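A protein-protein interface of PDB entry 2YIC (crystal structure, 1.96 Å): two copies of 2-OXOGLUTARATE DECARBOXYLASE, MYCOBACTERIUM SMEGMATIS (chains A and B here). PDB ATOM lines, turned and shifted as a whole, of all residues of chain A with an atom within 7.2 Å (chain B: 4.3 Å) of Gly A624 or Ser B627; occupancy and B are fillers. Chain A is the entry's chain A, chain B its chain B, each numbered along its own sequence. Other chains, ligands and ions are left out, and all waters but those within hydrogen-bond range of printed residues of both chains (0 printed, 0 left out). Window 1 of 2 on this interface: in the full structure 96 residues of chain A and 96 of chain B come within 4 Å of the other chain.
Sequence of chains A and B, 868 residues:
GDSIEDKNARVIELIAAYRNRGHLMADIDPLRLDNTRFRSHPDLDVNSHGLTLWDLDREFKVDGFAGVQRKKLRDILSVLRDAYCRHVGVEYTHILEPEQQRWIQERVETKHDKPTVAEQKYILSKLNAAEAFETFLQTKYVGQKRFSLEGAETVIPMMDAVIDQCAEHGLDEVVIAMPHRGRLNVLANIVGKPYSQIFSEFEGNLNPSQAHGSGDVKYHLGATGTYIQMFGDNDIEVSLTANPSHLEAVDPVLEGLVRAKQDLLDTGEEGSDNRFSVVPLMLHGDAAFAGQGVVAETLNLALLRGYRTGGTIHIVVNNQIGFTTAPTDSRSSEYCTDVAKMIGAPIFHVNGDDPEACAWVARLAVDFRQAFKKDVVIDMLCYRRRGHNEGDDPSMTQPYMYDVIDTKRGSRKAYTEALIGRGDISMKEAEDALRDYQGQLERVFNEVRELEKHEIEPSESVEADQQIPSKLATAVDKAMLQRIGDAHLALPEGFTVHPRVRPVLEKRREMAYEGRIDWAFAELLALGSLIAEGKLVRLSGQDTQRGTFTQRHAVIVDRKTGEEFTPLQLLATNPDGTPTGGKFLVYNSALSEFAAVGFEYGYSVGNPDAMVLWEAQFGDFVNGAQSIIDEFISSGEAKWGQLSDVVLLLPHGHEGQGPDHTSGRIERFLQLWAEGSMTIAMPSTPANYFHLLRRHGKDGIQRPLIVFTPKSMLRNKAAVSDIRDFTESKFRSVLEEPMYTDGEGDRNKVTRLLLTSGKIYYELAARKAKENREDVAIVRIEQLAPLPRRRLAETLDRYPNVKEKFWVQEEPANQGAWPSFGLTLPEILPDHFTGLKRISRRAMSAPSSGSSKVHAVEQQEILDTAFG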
ATOM      1  N   GLU A 297     -25.010  -9.547  15.649  1.00  0.00           N
ATOM      2  CA  GLU A 297     -26.316  -9.726  14.981  1.00  0.00           C
ATOM      3  C   GLU A 297     -27.428  -9.139  15.810  1.00  0.00           C
ATOM      4  O   GLU A 297     -28.351  -8.564  15.243  1.00  0.00           O
ATOM      5  CB  GLU A 297     -26.617 -11.215  14.749  1.00  0.00           C
ATOM      6  CG  GLU A 297     -25.784 -11.888  13.680  1.00  0.00           C
ATOM      7  CD  GLU A 297     -26.416 -13.144  13.091  1.00  0.00           C
ATOM      8  OE1 GLU A 297     -27.639 -13.330  13.282  1.00  0.00           O
ATOM      9  OE2 GLU A 297     -25.711 -13.917  12.400  1.00  0.00           O
ATOM     10  N   SER A 592     -30.039 -11.742   8.683  1.00  0.00           N
ATOM     11  CA  SER A 592     -29.588 -12.602   9.769  1.00  0.00           C
ATOM     12  C   SER A 592     -30.525 -13.792   9.879  1.00  0.00           C
ATOM     13  O   SER A 592     -31.716 -13.671   9.584  1.00  0.00           O
ATOM     14  CB  SER A 592     -29.580 -11.843  11.100  1.00  0.00           C
ATOM     15  OG  SER A 592     -28.986 -10.560  11.051  1.00  0.00           O
ATOM     16  N   GLU A 593     -29.987 -14.933  10.313  1.00  0.00           N
ATOM     17  CA  GLU A 593     -30.772 -16.130  10.589  1.00  0.00           C
ATOM     18  C   GLU A 593     -30.713 -16.383  12.085  1.00  0.00           C
ATOM     19  O   GLU A 593     -31.747 -16.434  12.733  1.00  0.00           O
ATOM     20  CB  GLU A 593     -30.289 -17.351   9.764  1.00  0.00           C
ATOM     21  CG  GLU A 593     -30.694 -17.277   8.295  1.00  0.00           C
ATOM     22  CD  GLU A 593     -29.788 -16.439   7.405  1.00  0.00           C
ATOM     23  OE1 GLU A 593     -28.590 -16.282   7.731  1.00  0.00           O
ATOM     24  OE2 GLU A 593     -30.282 -15.949   6.366  1.00  0.00           O
ATOM     25  N   PHE A 594     -29.508 -16.475  12.657  1.00  0.00           N
ATOM     26  CA  PHE A 594     -29.314 -16.734  14.089  1.00  0.00           C
ATOM     27  C   PHE A 594     -30.120 -15.746  14.959  1.00  0.00           C
ATOM     28  O   PHE A 594     -30.997 -16.183  15.699  1.00  0.00           O
ATOM     29  CB  PHE A 594     -27.799 -16.676  14.452  1.00  0.00           C
ATOM     30  CG  PHE A 594     -27.376 -17.363  15.749  1.00  0.00           C
ATOM     31  CD1 PHE A 594     -28.156 -17.269  16.897  1.00  0.00           C
ATOM     32  CD2 PHE A 594     -26.133 -17.981  15.852  1.00  0.00           C
ATOM     33  CE1 PHE A 594     -27.751 -17.873  18.101  1.00  0.00           C
ATOM     34  CE2 PHE A 594     -25.732 -18.592  17.049  1.00  0.00           C
ATOM     35  CZ  PHE A 594     -26.535 -18.515  18.174  1.00  0.00           C
ATOM     36  N   ALA A 595     -29.916 -14.449  14.805  1.00  0.00           N
ATOM     37  CA  ALA A 595     -30.650 -13.485  15.655  1.00  0.00           C
ATOM     38  C   ALA A 595     -32.117 -13.385  15.307  1.00  0.00           C
ATOM     39  O   ALA A 595     -32.924 -13.188  16.217  1.00  0.00           O
ATOM     40  CB  ALA A 595     -30.030 -12.108  15.578  1.00  0.00           C
ATOM     41  N   VAL A 597     -34.196 -15.730  14.031  1.00  0.00           N
ATOM     42  CA  VAL A 597     -34.922 -16.938  14.519  1.00  0.00           C
ATOM     43  C   VAL A 597     -35.002 -16.884  16.051  1.00  0.00           C
ATOM     44  O   VAL A 597     -36.054 -17.177  16.614  1.00  0.00           O
ATOM     45  CB  VAL A 597     -34.274 -18.249  13.997  1.00  0.00           C
ATOM     46  CG1 VAL A 597     -34.907 -19.498  14.602  1.00  0.00           C
ATOM     47  CG2 VAL A 597     -34.377 -18.315  12.473  1.00  0.00           C
ATOM     48  N   GLY A 619     -35.155 -22.520   2.696  1.00  0.00           N
ATOM     49  CA  GLY A 619     -34.896 -23.353   3.871  1.00  0.00           C
ATOM     50  C   GLY A 619     -33.421 -23.683   4.088  1.00  0.00           C
ATOM     51  O   GLY A 619     -32.994 -23.915   5.223  1.00  0.00           O
ATOM     52  N   ASP A 620     -32.618 -23.697   3.007  1.00  0.00           N
ATOM     53  CA  ASP A 620     -31.180 -24.012   3.031  1.00  0.00           C
ATOM     54  C   ASP A 620     -30.345 -23.051   3.943  1.00  0.00           C
ATOM     55  O   ASP A 620     -29.242 -23.410   4.352  1.00  0.00           O
ATOM     56  CB  ASP A 620     -30.622 -23.942   1.604  1.00  0.00           C
ATOM     57  CG  ASP A 620     -31.466 -24.636   0.553  1.00  0.00           C
ATOM     58  OD1 ASP A 620     -32.637 -24.241   0.376  1.00  0.00           O
ATOM     59  OD2 ASP A 620     -30.935 -25.531  -0.135  1.00  0.00           O
ATOM     60  N   PHE A 621     -30.867 -21.850   4.237  1.00  0.00           N
ATOM     61  CA  PHE A 621     -30.151 -20.860   5.039  1.00  0.00           C
ATOM     62  C   PHE A 621     -30.469 -20.965   6.516  1.00  0.00           C
ATOM     63  O   PHE A 621     -29.757 -20.362   7.333  1.00  0.00           O
ATOM     64  CB  PHE A 621     -30.416 -19.430   4.517  1.00  0.00           C
ATOM     65  CG  PHE A 621     -29.971 -19.275   3.093  1.00  0.00           C
ATOM     66  CD1 PHE A 621     -28.641 -19.492   2.737  1.00  0.00           C
ATOM     67  CD2 PHE A 621     -30.884 -18.986   2.088  1.00  0.00           C
ATOM     68  CE1 PHE A 621     -28.233 -19.413   1.410  1.00  0.00           C
ATOM     69  CE2 PHE A 621     -30.470 -18.885   0.758  1.00  0.00           C
ATOM     70  CZ  PHE A 621     -29.151 -19.114   0.425  1.00  0.00           C
ATOM     71  N   VAL A 622     -31.489 -21.769   6.883  1.00  0.00           N
ATOM     72  CA  VAL A 622     -31.866 -21.883   8.300  1.00  0.00           C
ATOM     73  C   VAL A 622     -30.739 -22.548   9.145  1.00  0.00           C
ATOM     74  O   VAL A 622     -30.723 -22.347  10.341  1.00  0.00           O
ATOM     75  CB  VAL A 622     -33.253 -22.555   8.524  1.00  0.00           C
ATOM     76  CG1 VAL A 622     -33.176 -24.080   8.444  1.00  0.00           C
ATOM     77  CG2 VAL A 622     -33.857 -22.112   9.863  1.00  0.00           C
ATOM     78  N   ASN A 623     -29.792 -23.279   8.534  1.00  0.00           N
ATOM     79  CA  ASN A 623     -28.676 -23.858   9.290  1.00  0.00           C
ATOM     80  C   ASN A 623     -27.790 -22.757   9.966  1.00  0.00           C
ATOM     81  O   ASN A 623     -27.082 -23.057  10.913  1.00  0.00           O
ATOM     82  CB  ASN A 623     -27.813 -24.810   8.446  1.00  0.00           C
ATOM     83  CG  ASN A 623     -27.246 -24.232   7.176  1.00  0.00           C
ATOM     84  OD1 ASN A 623     -27.602 -23.142   6.752  1.00  0.00           O
ATOM     85  ND2 ASN A 623     -26.392 -24.998   6.498  1.00  0.00           N
ATOM     86  N   GLY A 624     -27.912 -21.503   9.533  1.00  0.00           N
ATOM     87  CA  GLY A 624     -27.245 -20.377  10.171  1.00  0.00           C
ATOM     88  C   GLY A 624     -27.827 -20.111  11.540  1.00  0.00           C
ATOM     89  O   GLY A 624     -27.184 -19.491  12.374  1.00  0.00           O
ATOM     90  N   ALA A 625     -29.040 -20.643  11.808  1.00  0.00           N
ATOM     91  CA  ALA A 625     -29.720 -20.514  13.094  1.00  0.00           C
ATOM     92  C   ALA A 625     -29.774 -21.873  13.824  1.00  0.00           C
ATOM     93  O   ALA A 625     -30.625 -22.070  14.667  1.00  0.00           O
ATOM     94  CB  ALA A 625     -31.120 -19.991  12.878  1.00  0.00           C
ATOM     95  N   GLN A 626     -28.863 -22.801  13.504  1.00  0.00           N
ATOM     96  CA  GLN A 626     -28.875 -24.126  14.094  1.00  0.00           C
ATOM     97  C   GLN A 626     -28.868 -24.091  15.628  1.00  0.00           C
ATOM     98  O   GLN A 626     -29.636 -24.851  16.243  1.00  0.00           O
ATOM     99  CB  GLN A 626     -27.736 -25.004  13.582  1.00  0.00           C
ATOM    100  CG  GLN A 626     -28.001 -26.499  13.834  1.00  0.00           C
ATOM    101  CD  GLN A 626     -29.125 -27.003  12.958  1.00  0.00           C
ATOM    102  OE1 GLN A 626     -29.091 -26.856  11.735  1.00  0.00           O
ATOM    103  NE2 GLN A 626     -30.159 -27.550  13.570  1.00  0.00           N
ATOM    104  N   SER A 627     -28.043 -23.219  16.239  1.00  0.00           N
ATOM    105  CA  SER A 627     -27.969 -23.146  17.696  1.00  0.00           C
ATOM    106  C   SER A 627     -29.344 -22.874  18.275  1.00  0.00           C
ATOM    107  O   SER A 627     -29.687 -23.469  19.274  1.00  0.00           O
ATOM    108  CB  SER A 627     -26.994 -22.060  18.160  1.00  0.00           C
ATOM    109  OG  SER A 627     -25.668 -22.302  17.729  1.00  0.00           O
ATOM    110  N   ILE A 628     -30.135 -21.998  17.625  1.00  0.00           N
ATOM    111  CA  ILE A 628     -31.460 -21.671  18.168  1.00  0.00           C
ATOM    112  C   ILE A 628     -32.389 -22.836  17.978  1.00  0.00           C
ATOM    113  O   ILE A 628     -33.223 -23.088  18.838  1.00  0.00           O
ATOM    114  CB  ILE A 628     -32.078 -20.380  17.561  1.00  0.00           C
ATOM    115  CG1 ILE A 628     -31.185 -19.119  17.804  1.00  0.00           C
ATOM    116  CG2 ILE A 628     -33.540 -20.172  18.062  1.00  0.00           C
ATOM    117  CD1 ILE A 628     -31.094 -18.561  19.295  1.00  0.00           C
ATOM    118  N   ILE A 629     -32.288 -23.526  16.835  1.00  0.00           N
ATOM    119  CA  ILE A 629     -33.172 -24.664  16.591  1.00  0.00           C
ATOM    120  C   ILE A 629     -32.863 -25.782  17.598  1.00  0.00           C
ATOM    121  O   ILE A 629     -33.780 -26.353  18.162  1.00  0.00           O
ATOM    122  CB  ILE A 629     -33.050 -25.140  15.123  1.00  0.00           C
ATOM    123  CG1 ILE A 629     -33.589 -24.035  14.131  1.00  0.00           C
ATOM    124  CG2 ILE A 629     -33.736 -26.515  14.900  1.00  0.00           C
ATOM    125  CD1 ILE A 629     -33.110 -24.319  12.662  1.00  0.00           C
ATOM    126  N   ARG A 668     -33.119 -33.433   9.228  1.00  0.00           N
ATOM    127  CA  ARG A 668     -32.544 -32.899  10.452  1.00  0.00           C
ATOM    128  C   ARG A 668     -33.640 -32.566  11.463  1.00  0.00           C
ATOM    129  O   ARG A 668     -33.492 -32.881  12.649  1.00  0.00           O
ATOM    130  CB  ARG A 668     -31.664 -31.674  10.159  1.00  0.00           C
ATOM    131  CG  ARG A 668     -30.811 -31.223  11.375  1.00  0.00           C
ATOM    132  CD  ARG A 668     -29.805 -30.147  10.950  1.00  0.00           C
ATOM    133  NE  ARG A 668     -28.779 -30.716  10.063  1.00  0.00           N
ATOM    134  CZ  ARG A 668     -27.857 -30.007   9.424  1.00  0.00           C
ATOM    135  NH1 ARG A 668     -27.821 -28.691   9.547  1.00  0.00           N
ATOM    136  NH2 ARG A 668     -26.967 -30.607   8.655  1.00  0.00           N
ATOM    137  N   PHE B 594     -18.128 -20.833  14.757  1.00  0.00           N
ATOM    138  CA  PHE B 594     -18.283 -20.538  13.314  1.00  0.00           C
ATOM    139  C   PHE B 594     -16.952 -20.068  12.685  1.00  0.00           C
ATOM    140  O   PHE B 594     -16.434 -20.731  11.779  1.00  0.00           O
ATOM    141  CB  PHE B 594     -19.366 -19.449  13.119  1.00  0.00           C
ATOM    142  CG  PHE B 594     -20.001 -19.297  11.756  1.00  0.00           C
ATOM    143  CD1 PHE B 594     -19.260 -19.492  10.590  1.00  0.00           C
ATOM    144  CD2 PHE B 594     -21.337 -18.922  11.635  1.00  0.00           C
ATOM    145  CE1 PHE B 594     -19.858 -19.348   9.320  1.00  0.00           C
ATOM    146  CE2 PHE B 594     -21.931 -18.776  10.364  1.00  0.00           C
ATOM    147  CZ  PHE B 594     -21.181 -18.988   9.218  1.00  0.00           C
ATOM    148  N   ALA B 625     -21.129 -23.833  14.530  1.00  0.00           N
ATOM    149  CA  ALA B 625     -20.406 -23.863  13.254  1.00  0.00           C
ATOM    150  C   ALA B 625     -21.154 -24.715  12.212  1.00  0.00           C
ATOM    151  O   ALA B 625     -20.540 -25.195  11.248  1.00  0.00           O
ATOM    152  CB  ALA B 625     -19.017 -24.443  13.497  1.00  0.00           C
ATOM    153  N   GLN B 626     -22.481 -24.915  12.387  1.00  0.00           N
ATOM    154  CA  GLN B 626     -23.246 -25.776  11.462  1.00  0.00           C
ATOM    155  C   GLN B 626     -23.112 -25.339   9.997  1.00  0.00           C
ATOM    156  O   GLN B 626     -22.949 -26.204   9.117  1.00  0.00           O
ATOM    157  CB  GLN B 626     -24.734 -25.850  11.841  1.00  0.00           C
ATOM    158  CG  GLN B 626     -25.432 -27.053  11.186  1.00  0.00           C
ATOM    159  CD  GLN B 626     -24.930 -28.346  11.790  1.00  0.00           C
ATOM    160  OE1 GLN B 626     -24.972 -28.535  13.006  1.00  0.00           O
ATOM    161  NE2 GLN B 626     -24.418 -29.246  10.955  1.00  0.00           N
ATOM    162  N   SER B 627     -23.157 -24.018   9.724  1.00  0.00           N
ATOM    163  CA  SER B 627     -23.029 -23.560   8.319  1.00  0.00           C
ATOM    164  C   SER B 627     -21.709 -24.056   7.705  1.00  0.00           C
ATOM    165  O   SER B 627     -21.712 -24.461   6.560  1.00  0.00           O
ATOM    166  CB  SER B 627     -23.094 -22.037   8.226  1.00  0.00           C
ATOM    167  OG  SER B 627     -24.348 -21.541   8.667  1.00  0.00           O
ATOM    168  N   ILE B 628     -20.593 -24.052   8.468  1.00  0.00           N
ATOM    169  CA  ILE B 628     -19.300 -24.514   7.921  1.00  0.00           C
ATOM    170  C   ILE B 628     -19.343 -26.010   7.717  1.00  0.00           C
ATOM    171  O   ILE B 628     -18.845 -26.507   6.699  1.00  0.00           O
ATOM    172  CB  ILE B 628     -18.088 -24.076   8.820  1.00  0.00           C
ATOM    173  CG1 ILE B 628     -18.008 -22.534   8.988  1.00  0.00           C
ATOM    174  CG2 ILE B 628     -16.731 -24.665   8.311  1.00  0.00           C
ATOM    175  CD1 ILE B 628     -17.720 -21.667   7.635  1.00  0.00           C
ATOM    176  N   ILE B 629     -19.900 -26.743   8.697  1.00  0.00           N
ATOM    177  CA  ILE B 629     -20.009 -28.202   8.591  1.00  0.00           C
ATOM    178  C   ILE B 629     -20.830 -28.562   7.336  1.00  0.00           C
ATOM    179  O   ILE B 629     -20.340 -29.305   6.489  1.00  0.00           O
ATOM    180  CB  ILE B 629     -20.591 -28.853   9.868  1.00  0.00           C
ATOM    181  CG1 ILE B 629     -19.587 -28.759  11.037  1.00  0.00           C
ATOM    182  CG2 ILE B 629     -20.947 -30.339   9.600  1.00  0.00           C
ATOM    183  CD1 ILE B 629     -20.249 -28.871  12.429  1.00  0.00           C
ATOM    184  N   ASP B 630     -22.031 -27.967   7.181  1.00  0.00           N
ATOM    185  CA  ASP B 630     -22.908 -28.266   6.047  1.00  0.00           C
ATOM    186  C   ASP B 630     -22.377 -27.804   4.693  1.00  0.00           C
ATOM    187  O   ASP B 630     -22.446 -28.546   3.731  1.00  0.00           O
ATOM    188  CB  ASP B 630     -24.279 -27.595   6.268  1.00  0.00           C
ATOM    189  CG  ASP B 630     -25.087 -28.093   7.443  1.00  0.00           C
ATOM    190  OD1 ASP B 630     -24.687 -29.122   8.057  1.00  0.00           O
ATOM    191  OD2 ASP B 630     -26.131 -27.466   7.747  1.00  0.00           O
ATOM    192  N   GLU B 631     -21.891 -26.563   4.611  1.00  0.00           N
ATOM    193  CA  GLU B 631     -21.547 -25.925   3.339  1.00  0.00           C
ATOM    194  C   GLU B 631     -20.137 -26.137   2.868  1.00  0.00           C
ATOM    195  O   GLU B 631     -19.914 -25.975   1.682  1.00  0.00           O
ATOM    196  CB  GLU B 631     -21.814 -24.400   3.437  1.00  0.00           C
ATOM    197  CG  GLU B 631     -23.256 -24.065   3.794  1.00  0.00           C
ATOM    198  CD  GLU B 631     -24.267 -24.650   2.824  1.00  0.00           C
ATOM    199  OE1 GLU B 631     -24.028 -24.587   1.593  1.00  0.00           O
ATOM    200  OE2 GLU B 631     -25.291 -25.189   3.298  1.00  0.00           O
ATOM    201  N   PHE B 632     -19.190 -26.475   3.767  1.00  0.00           N
ATOM    202  CA  PHE B 632     -17.799 -26.620   3.349  1.00  0.00           C
ATOM    203  C   PHE B 632     -17.248 -27.991   3.635  1.00  0.00           C
ATOM    204  O   PHE B 632     -16.886 -28.704   2.702  1.00  0.00           O
ATOM    205  CB  PHE B 632     -16.922 -25.565   4.043  1.00  0.00           C
ATOM    206  CG  PHE B 632     -17.103 -24.145   3.589  1.00  0.00           C
ATOM    207  CD1 PHE B 632     -16.372 -23.643   2.512  1.00  0.00           C
ATOM    208  CD2 PHE B 632     -17.922 -23.270   4.302  1.00  0.00           C
ATOM    209  CE1 PHE B 632     -16.505 -22.306   2.110  1.00  0.00           C
ATOM    210  CE2 PHE B 632     -18.059 -21.926   3.890  1.00  0.00           C
ATOM    211  CZ  PHE B 632     -17.322 -21.449   2.819  1.00  0.00           C
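OD1 of Asn A623 lies close to O of Asp A620. NH1 of Arg A668 lies within hydrogen-bond range of OE1 of Gln A626 (3.1 Å). The side-chain amide nitrogen (NE2) of Gln B626 is in hydrogen-bond range of the side-chain carboxylate (OD1) of Asp B630, 2.9 Å away.
Of the 18 printed residues of chain A, 4 touch a printed residue of chain B. Among the printed residues, 8 pairs touch across the chains. Among the printed residues, Asp or Glu carboxylates within 4 Å of a Lys or Arg side-chain nitrogen of the other chain: Arg A668 with Asp B630 (2.8 Å).
Glu A297 touches none of the printed residues of chain B. Ala A595 touches none of the printed residues of chain B. Of the printed residues of chain B, Asn A623 touches Gln B626, Ser B627, Asp B630 and Glu B631. Gly A624 touches just one residue of chain B: Ser B627. Of the printed residues of chain B, Gln A626 touches Gln B626. Of the printed residues of chain B, Arg A668 touches Gln B626 (3.3 Å) and Asp B630 (2.8 Å). Of the printed residues of chain A, Ser B627 touches Asn A623 and Gly A624. Of the printed residues of chain A, Asp B630 touches Asn A623 and Arg A668.
Gln B626 touches its own counterpart, Gln A626.
ND2 of Asn A623 lies within hydrogen-bond range of OD2 of Asp B630. The side-chain amide nitrogen (ND2) of Asn A623 lies within hydrogen-bond range of the side-chain carboxylate (OE2) of Glu B631 (3.4 Å). The side-chain carboxylate (OD2) of Asp B630 lies within salt-bridge range of the guanidinium group (NH1) of Arg A668, 2.8 Å away.
Gln B626 touches Asn A623. O of Asn A623 touches OG of Ser B627 (3.8 Å). Ser B627 touches Gly A624 (OG to CA, 3.5 Å). CB of Gln A626 touches CB of Gln B626, 3.6 Å away. NH1 of Arg A668 touches CG of Gln B626 (3.3 Å).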
